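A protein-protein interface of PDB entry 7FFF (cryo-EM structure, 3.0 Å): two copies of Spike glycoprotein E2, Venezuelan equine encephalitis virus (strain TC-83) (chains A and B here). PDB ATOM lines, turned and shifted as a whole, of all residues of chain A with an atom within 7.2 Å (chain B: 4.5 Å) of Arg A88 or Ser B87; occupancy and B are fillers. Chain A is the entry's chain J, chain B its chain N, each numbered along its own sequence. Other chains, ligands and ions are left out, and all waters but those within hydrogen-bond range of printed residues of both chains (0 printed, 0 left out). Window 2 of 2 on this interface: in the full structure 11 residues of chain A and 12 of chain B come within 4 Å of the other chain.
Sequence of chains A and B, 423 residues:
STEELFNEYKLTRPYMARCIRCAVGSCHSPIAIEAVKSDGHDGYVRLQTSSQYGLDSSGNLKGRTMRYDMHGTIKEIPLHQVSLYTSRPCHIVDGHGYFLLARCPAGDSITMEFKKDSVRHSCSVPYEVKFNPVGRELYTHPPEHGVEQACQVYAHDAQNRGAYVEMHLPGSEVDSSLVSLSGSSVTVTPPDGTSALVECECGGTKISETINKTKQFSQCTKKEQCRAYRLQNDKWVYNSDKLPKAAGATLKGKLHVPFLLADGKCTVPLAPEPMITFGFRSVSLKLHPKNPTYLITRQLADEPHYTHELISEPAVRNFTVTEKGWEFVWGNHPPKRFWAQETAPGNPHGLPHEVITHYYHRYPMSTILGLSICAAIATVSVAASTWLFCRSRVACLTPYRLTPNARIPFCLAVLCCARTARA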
ATOM      1  N   LEU A  84      29.692  11.939  -4.719  1.00  0.00           N
ATOM      2  CA  LEU A  84      29.322  12.037  -6.120  1.00  0.00           C
ATOM      3  C   LEU A  84      27.910  11.508  -6.306  1.00  0.00           C
ATOM      4  O   LEU A  84      27.326  10.902  -5.409  1.00  0.00           O
ATOM      5  CB  LEU A  84      30.309  11.319  -7.043  1.00  0.00           C
ATOM      6  CG  LEU A  84      30.299   9.823  -7.291  1.00  0.00           C
ATOM      7  CD1 LEU A  84      31.068   9.554  -8.552  1.00  0.00           C
ATOM      8  CD2 LEU A  84      30.954   9.137  -6.160  1.00  0.00           C
ATOM      9  N   TYR A  85      27.361  11.774  -7.489  1.00  0.00           N
ATOM     10  CA  TYR A  85      25.984  11.431  -7.798  1.00  0.00           C
ATOM     11  C   TYR A  85      25.828  11.318  -9.308  1.00  0.00           C
ATOM     12  O   TYR A  85      26.644  11.836 -10.069  1.00  0.00           O
ATOM     13  CB  TYR A  85      25.013  12.455  -7.198  1.00  0.00           C
ATOM     14  CG  TYR A  85      25.205  13.891  -7.603  1.00  0.00           C
ATOM     15  CD1 TYR A  85      26.014  14.737  -6.861  1.00  0.00           C
ATOM     16  CD2 TYR A  85      24.546  14.415  -8.699  1.00  0.00           C
ATOM     17  CE1 TYR A  85      26.182  16.049  -7.214  1.00  0.00           C
ATOM     18  CE2 TYR A  85      24.713  15.728  -9.063  1.00  0.00           C
ATOM     19  CZ  TYR A  85      25.529  16.539  -8.315  1.00  0.00           C
ATOM     20  OH  TYR A  85      25.688  17.851  -8.674  1.00  0.00           O
ATOM     21  N   THR A  86      24.799  10.580  -9.729  1.00  0.00           N
ATOM     22  CA  THR A  86      24.417  10.488 -11.137  1.00  0.00           C
ATOM     23  C   THR A  86      23.042  11.092 -11.381  1.00  0.00           C
ATOM     24  O   THR A  86      22.913  12.033 -12.166  1.00  0.00           O
ATOM     25  CB  THR A  86      24.410   9.028 -11.601  1.00  0.00           C
ATOM     26  OG1 THR A  86      23.476   8.301 -10.804  1.00  0.00           O
ATOM     27  CG2 THR A  86      25.740   8.409 -11.423  1.00  0.00           C
ATOM     28  N   SER A  87      22.031  10.568 -10.749  1.00  0.00           N
ATOM     29  CA  SER A  87      20.712  11.153 -10.591  1.00  0.00           C
ATOM     30  C   SER A  87      20.281  11.125  -9.138  1.00  0.00           C
ATOM     31  O   SER A  87      19.656  12.070  -8.660  1.00  0.00           O
ATOM     32  CB  SER A  87      19.716  10.395 -11.458  1.00  0.00           C
ATOM     33  OG  SER A  87      20.083  10.489 -12.819  1.00  0.00           O
ATOM     34  N   ARG A  88      20.611  10.061  -8.433  1.00  0.00           N
ATOM     35  CA  ARG A  88      20.574   9.900  -6.997  1.00  0.00           C
ATOM     36  C   ARG A  88      21.989  10.032  -6.466  1.00  0.00           C
ATOM     37  O   ARG A  88      22.953   9.995  -7.236  1.00  0.00           O
ATOM     38  CB  ARG A  88      20.015   8.518  -6.652  1.00  0.00           C
ATOM     39  CG  ARG A  88      18.571   8.302  -6.963  1.00  0.00           C
ATOM     40  CD  ARG A  88      18.216   6.859  -6.689  1.00  0.00           C
ATOM     41  NE  ARG A  88      16.805   6.611  -6.918  1.00  0.00           N
ATOM     42  CZ  ARG A  88      16.288   6.283  -8.092  1.00  0.00           C
ATOM     43  NH1 ARG A  88      14.982   6.072  -8.204  1.00  0.00           N
ATOM     44  NH2 ARG A  88      17.073   6.171  -9.155  1.00  0.00           N
ATOM     45  N   PRO A  89      22.166  10.203  -5.156  1.00  0.00           N
ATOM     46  CA  PRO A  89      23.517  10.121  -4.592  1.00  0.00           C
ATOM     47  C   PRO A  89      24.084   8.713  -4.674  1.00  0.00           C
ATOM     48  O   PRO A  89      23.379   7.726  -4.462  1.00  0.00           O
ATOM     49  CB  PRO A  89      23.316  10.552  -3.137  1.00  0.00           C
ATOM     50  CG  PRO A  89      22.137  11.395  -3.175  1.00  0.00           C
ATOM     51  CD  PRO A  89      21.233  10.800  -4.189  1.00  0.00           C
ATOM     52  N   CYS A  90      25.365   8.633  -5.013  1.00  0.00           N
ATOM     53  CA  CYS A  90      26.099   7.380  -5.016  1.00  0.00           C
ATOM     54  C   CYS A  90      26.735   7.153  -3.648  1.00  0.00           C
ATOM     55  O   CYS A  90      26.549   7.932  -2.711  1.00  0.00           O
ATOM     56  CB  CYS A  90      27.173   7.386  -6.097  1.00  0.00           C
ATOM     57  SG  CYS A  90      26.576   7.475  -7.770  1.00  0.00           S
ATOM     58  N   HIS A  91      27.501   6.071  -3.524  1.00  0.00           N
ATOM     59  CA  HIS A  91      28.169   5.729  -2.272  1.00  0.00           C
ATOM     60  C   HIS A  91      29.559   5.204  -2.596  1.00  0.00           C
ATOM     61  O   HIS A  91      29.688   4.137  -3.196  1.00  0.00           O
ATOM     62  CB  HIS A  91      27.371   4.696  -1.482  1.00  0.00           C
ATOM     63  CG  HIS A  91      26.082   5.219  -0.936  1.00  0.00           C
ATOM     64  ND1 HIS A  91      24.883   5.081  -1.595  1.00  0.00           N
ATOM     65  CD2 HIS A  91      25.809   5.895   0.202  1.00  0.00           C
ATOM     66  CE1 HIS A  91      23.923   5.642  -0.883  1.00  0.00           C
ATOM     67  NE2 HIS A  91      24.460   6.145   0.213  1.00  0.00           N
ATOM     68  N   CYS A 104      26.806   3.238  -7.788  1.00  0.00           N
ATOM     69  CA  CYS A 104      25.990   4.267  -8.396  1.00  0.00           C
ATOM     70  C   CYS A 104      24.733   3.695  -9.033  1.00  0.00           C
ATOM     71  O   CYS A 104      24.736   2.569  -9.534  1.00  0.00           O
ATOM     72  CB  CYS A 104      26.788   5.024  -9.454  1.00  0.00           C
ATOM     73  SG  CYS A 104      27.855   6.277  -8.782  1.00  0.00           S
ATOM     74  N   PRO A 105      23.644   4.455  -9.020  1.00  0.00           N
ATOM     75  CA  PRO A 105      22.477   4.118  -9.827  1.00  0.00           C
ATOM     76  C   PRO A 105      22.685   4.616 -11.249  1.00  0.00           C
ATOM     77  O   PRO A 105      23.684   5.247 -11.569  1.00  0.00           O
ATOM     78  CB  PRO A 105      21.354   4.879  -9.140  1.00  0.00           C
ATOM     79  CG  PRO A 105      22.027   6.070  -8.618  1.00  0.00           C
ATOM     80  CD  PRO A 105      23.385   5.631  -8.176  1.00  0.00           C
ATOM     81  N   ALA A 106      21.714   4.328 -12.102  1.00  0.00           N
ATOM     82  CA  ALA A 106      21.835   4.695 -13.498  1.00  0.00           C
ATOM     83  C   ALA A 106      21.619   6.190 -13.694  1.00  0.00           C
ATOM     84  O   ALA A 106      20.887   6.840 -12.947  1.00  0.00           O
ATOM     85  CB  ALA A 106      20.840   3.913 -14.346  1.00  0.00           C
ATOM     86  N   GLY A 107      22.270   6.727 -14.712  1.00  0.00           N
ATOM     87  CA  GLY A 107      22.053   8.107 -15.082  1.00  0.00           C
ATOM     88  C   GLY A 107      22.831   8.417 -16.335  1.00  0.00           C
ATOM     89  O   GLY A 107      23.342   7.523 -17.003  1.00  0.00           O
ATOM     90  N   THR A 140      15.656  -2.669 -10.423  1.00  0.00           N
ATOM     91  CA  THR A 140      16.472  -1.465 -10.438  1.00  0.00           C
ATOM     92  C   THR A 140      17.220  -1.270  -9.130  1.00  0.00           C
ATOM     93  O   THR A 140      18.310  -0.692  -9.130  1.00  0.00           O
ATOM     94  CB  THR A 140      15.592  -0.242 -10.731  1.00  0.00           C
ATOM     95  OG1 THR A 140      14.785  -0.523 -11.875  1.00  0.00           O
ATOM     96  CG2 THR A 140      16.417   0.976 -11.069  1.00  0.00           C
ATOM     97  N   TYR B  85      15.328  10.142   1.152  1.00  0.00           N
ATOM     98  CA  TYR B  85      15.052  10.515  -0.225  1.00  0.00           C
ATOM     99  C   TYR B  85      14.643   9.281  -1.010  1.00  0.00           C
ATOM    100  O   TYR B  85      15.175   8.197  -0.782  1.00  0.00           O
ATOM    101  CB  TYR B  85      16.272  11.185  -0.867  1.00  0.00           C
ATOM    102  CG  TYR B  85      17.526  10.358  -0.883  1.00  0.00           C
ATOM    103  CD1 TYR B  85      18.399  10.367   0.195  1.00  0.00           C
ATOM    104  CD2 TYR B  85      17.869   9.612  -1.995  1.00  0.00           C
ATOM    105  CE1 TYR B  85      19.550   9.623   0.180  1.00  0.00           C
ATOM    106  CE2 TYR B  85      19.020   8.864  -2.017  1.00  0.00           C
ATOM    107  CZ  TYR B  85      19.855   8.876  -0.929  1.00  0.00           C
ATOM    108  OH  TYR B  85      21.001   8.128  -0.963  1.00  0.00           O
ATOM    109  N   THR B  86      13.689   9.450  -1.924  1.00  0.00           N
ATOM    110  CA  THR B  86      13.262   8.375  -2.817  1.00  0.00           C
ATOM    111  C   THR B  86      13.945   8.450  -4.177  1.00  0.00           C
ATOM    112  O   THR B  86      14.675   7.537  -4.563  1.00  0.00           O
ATOM    113  CB  THR B  86      11.750   8.428  -2.992  1.00  0.00           C
ATOM    114  OG1 THR B  86      11.397   9.672  -3.596  1.00  0.00           O
ATOM    115  CG2 THR B  86      11.078   8.344  -1.665  1.00  0.00           C
ATOM    116  N   SER B  87      13.715   9.511  -4.905  1.00  0.00           N
ATOM    117  CA  SER B  87      14.440   9.894  -6.109  1.00  0.00           C
ATOM    118  C   SER B  87      15.013  11.291  -5.992  1.00  0.00           C
ATOM    119  O   SER B  87      16.107  11.552  -6.493  1.00  0.00           O
ATOM    120  CB  SER B  87      13.537   9.839  -7.336  1.00  0.00           C
ATOM    121  OG  SER B  87      13.150   8.514  -7.617  1.00  0.00           O
ATOM    122  N   ARG B  88      14.284  12.189  -5.364  1.00  0.00           N
ATOM    123  CA  ARG B  88      14.656  13.539  -5.007  1.00  0.00           C
ATOM    124  C   ARG B  88      14.529  13.573  -3.490  1.00  0.00           C
ATOM    125  O   ARG B  88      13.984  12.618  -2.928  1.00  0.00           O
ATOM    126  CB  ARG B  88      13.742  14.534  -5.716  1.00  0.00           C
ATOM    127  CG  ARG B  88      13.958  14.528  -7.208  1.00  0.00           C
ATOM    128  CD  ARG B  88      13.133  15.562  -7.915  1.00  0.00           C
ATOM    129  NE  ARG B  88      11.729  15.214  -8.007  1.00  0.00           N
ATOM    130  CZ  ARG B  88      10.770  15.886  -7.390  1.00  0.00           C
ATOM    131  NH1 ARG B  88      11.087  16.926  -6.634  1.00  0.00           N
ATOM    132  NH2 ARG B  88       9.505  15.527  -7.526  1.00  0.00           N
ATOM    133  N   ALA B 106       7.899  10.316  -5.953  1.00  0.00           N
ATOM    134  CA  ALA B 106       7.892   8.902  -6.285  1.00  0.00           C
ATOM    135  C   ALA B 106       9.298   8.396  -6.568  1.00  0.00           C
ATOM    136  O   ALA B 106      10.172   9.140  -7.017  1.00  0.00           O
ATOM    137  CB  ALA B 106       7.007   8.643  -7.498  1.00  0.00           C
ATOM    138  N   GLY B 107       9.501   7.109  -6.325  1.00  0.00           N
ATOM    139  CA  GLY B 107      10.780   6.493  -6.623  1.00  0.00           C
ATOM    140  C   GLY B 107      10.691   4.997  -6.464  1.00  0.00           C
ATOM    141  O   GLY B 107       9.640   4.447  -6.142  1.00  0.00           O
ATOM    142  N   ASP B 108      11.823   4.340  -6.693  1.00  0.00           N
ATOM    143  CA  ASP B 108      11.898   2.890  -6.583  1.00  0.00           C
ATOM    144  C   ASP B 108      12.266   2.423  -5.185  1.00  0.00           C
ATOM    145  O   ASP B 108      11.911   1.306  -4.802  1.00  0.00           O
ATOM    146  CB  ASP B 108      12.936   2.338  -7.557  1.00  0.00           C
ATOM    147  CG  ASP B 108      12.585   2.613  -8.989  1.00  0.00           C
ATOM    148  OD1 ASP B 108      11.377   2.711  -9.292  1.00  0.00           O
ATOM    149  OD2 ASP B 108      13.517   2.744  -9.809  1.00  0.00           O
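The backbone carbonyl oxygen of Thr B86 lies within hydrogen-bond range of the guanidinium group of Arg A88, 3.3 Å away. The guanidinium group of Arg A88 sits at hydrogen-bond distance from the side-chain hydroxyl of Ser B87, at 3.1 Å. OD2 of Asp B108 lies within salt-bridge range of NH1 of Arg A88, 3.97 Å away.
OG of Ser B87 sits at hydrogen-bond distance from O of Ala B106, at 3.1 Å. The side-chain sulfur (SG) of Cys A90 forms a disulfide with the side-chain sulfur (SG) of Cys A104 (2.0 Å).
Among the printed residues, pairs that only touch across the chains: Thr A140 with Asp B108, Pro A89 with Tyr B85 and His A91 with Tyr B85.
Arg A88 touches just these residues of chain B: Thr B86 (3.3 Å), Ser B87 (3.1 Å) and Asp B108 (3.9 Å). Of the printed residues of chain B, His A91 touches Tyr B85 (3.8 Å). Printed residues of chain B within 4 Å of Thr A140: Asp B108. Printed residues of chain A within 4 Å of Ser B87: Arg A88 (3.1 Å). Arg B88 touches none of the printed residues of chain A. Printed residues of chain A within 4 Å of Asp B108: Arg A88 (3.9 Å) and Thr A140 (3.6 Å). The nearest printed residue of chain B that does not touch Arg A88 is Gly B107 (4.5 Å). The nearest printed residue of chain A that does not touch Tyr B85 is Arg A88 (4.8 Å).
Of the 13 printed residues of chain A, 4 touch a printed residue of chain B. Printed residues of chain A that touch a printed residue of chain B: Arg A88, Pro A89, His A91 and Thr A140. Of the 7 printed residues of chain B, 4 touch a printed residue of chain A. Among the printed residues, 6 pairs touch across the chains.
Arg A88 touches Thr B86, but with the chains exchanged Thr A86 does not touch Arg B88 (10.5 Å). Arg A88 touches Ser B87, but with the chains exchanged Ser A87 does not touch Arg B88 (6.3 Å). Positions printed for both chains: 85, 86, 87, 88, 106 and 107. Of the 6 pairs that touch across the chains among the printed residues, none has its exchanged pair printed and touching as well.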
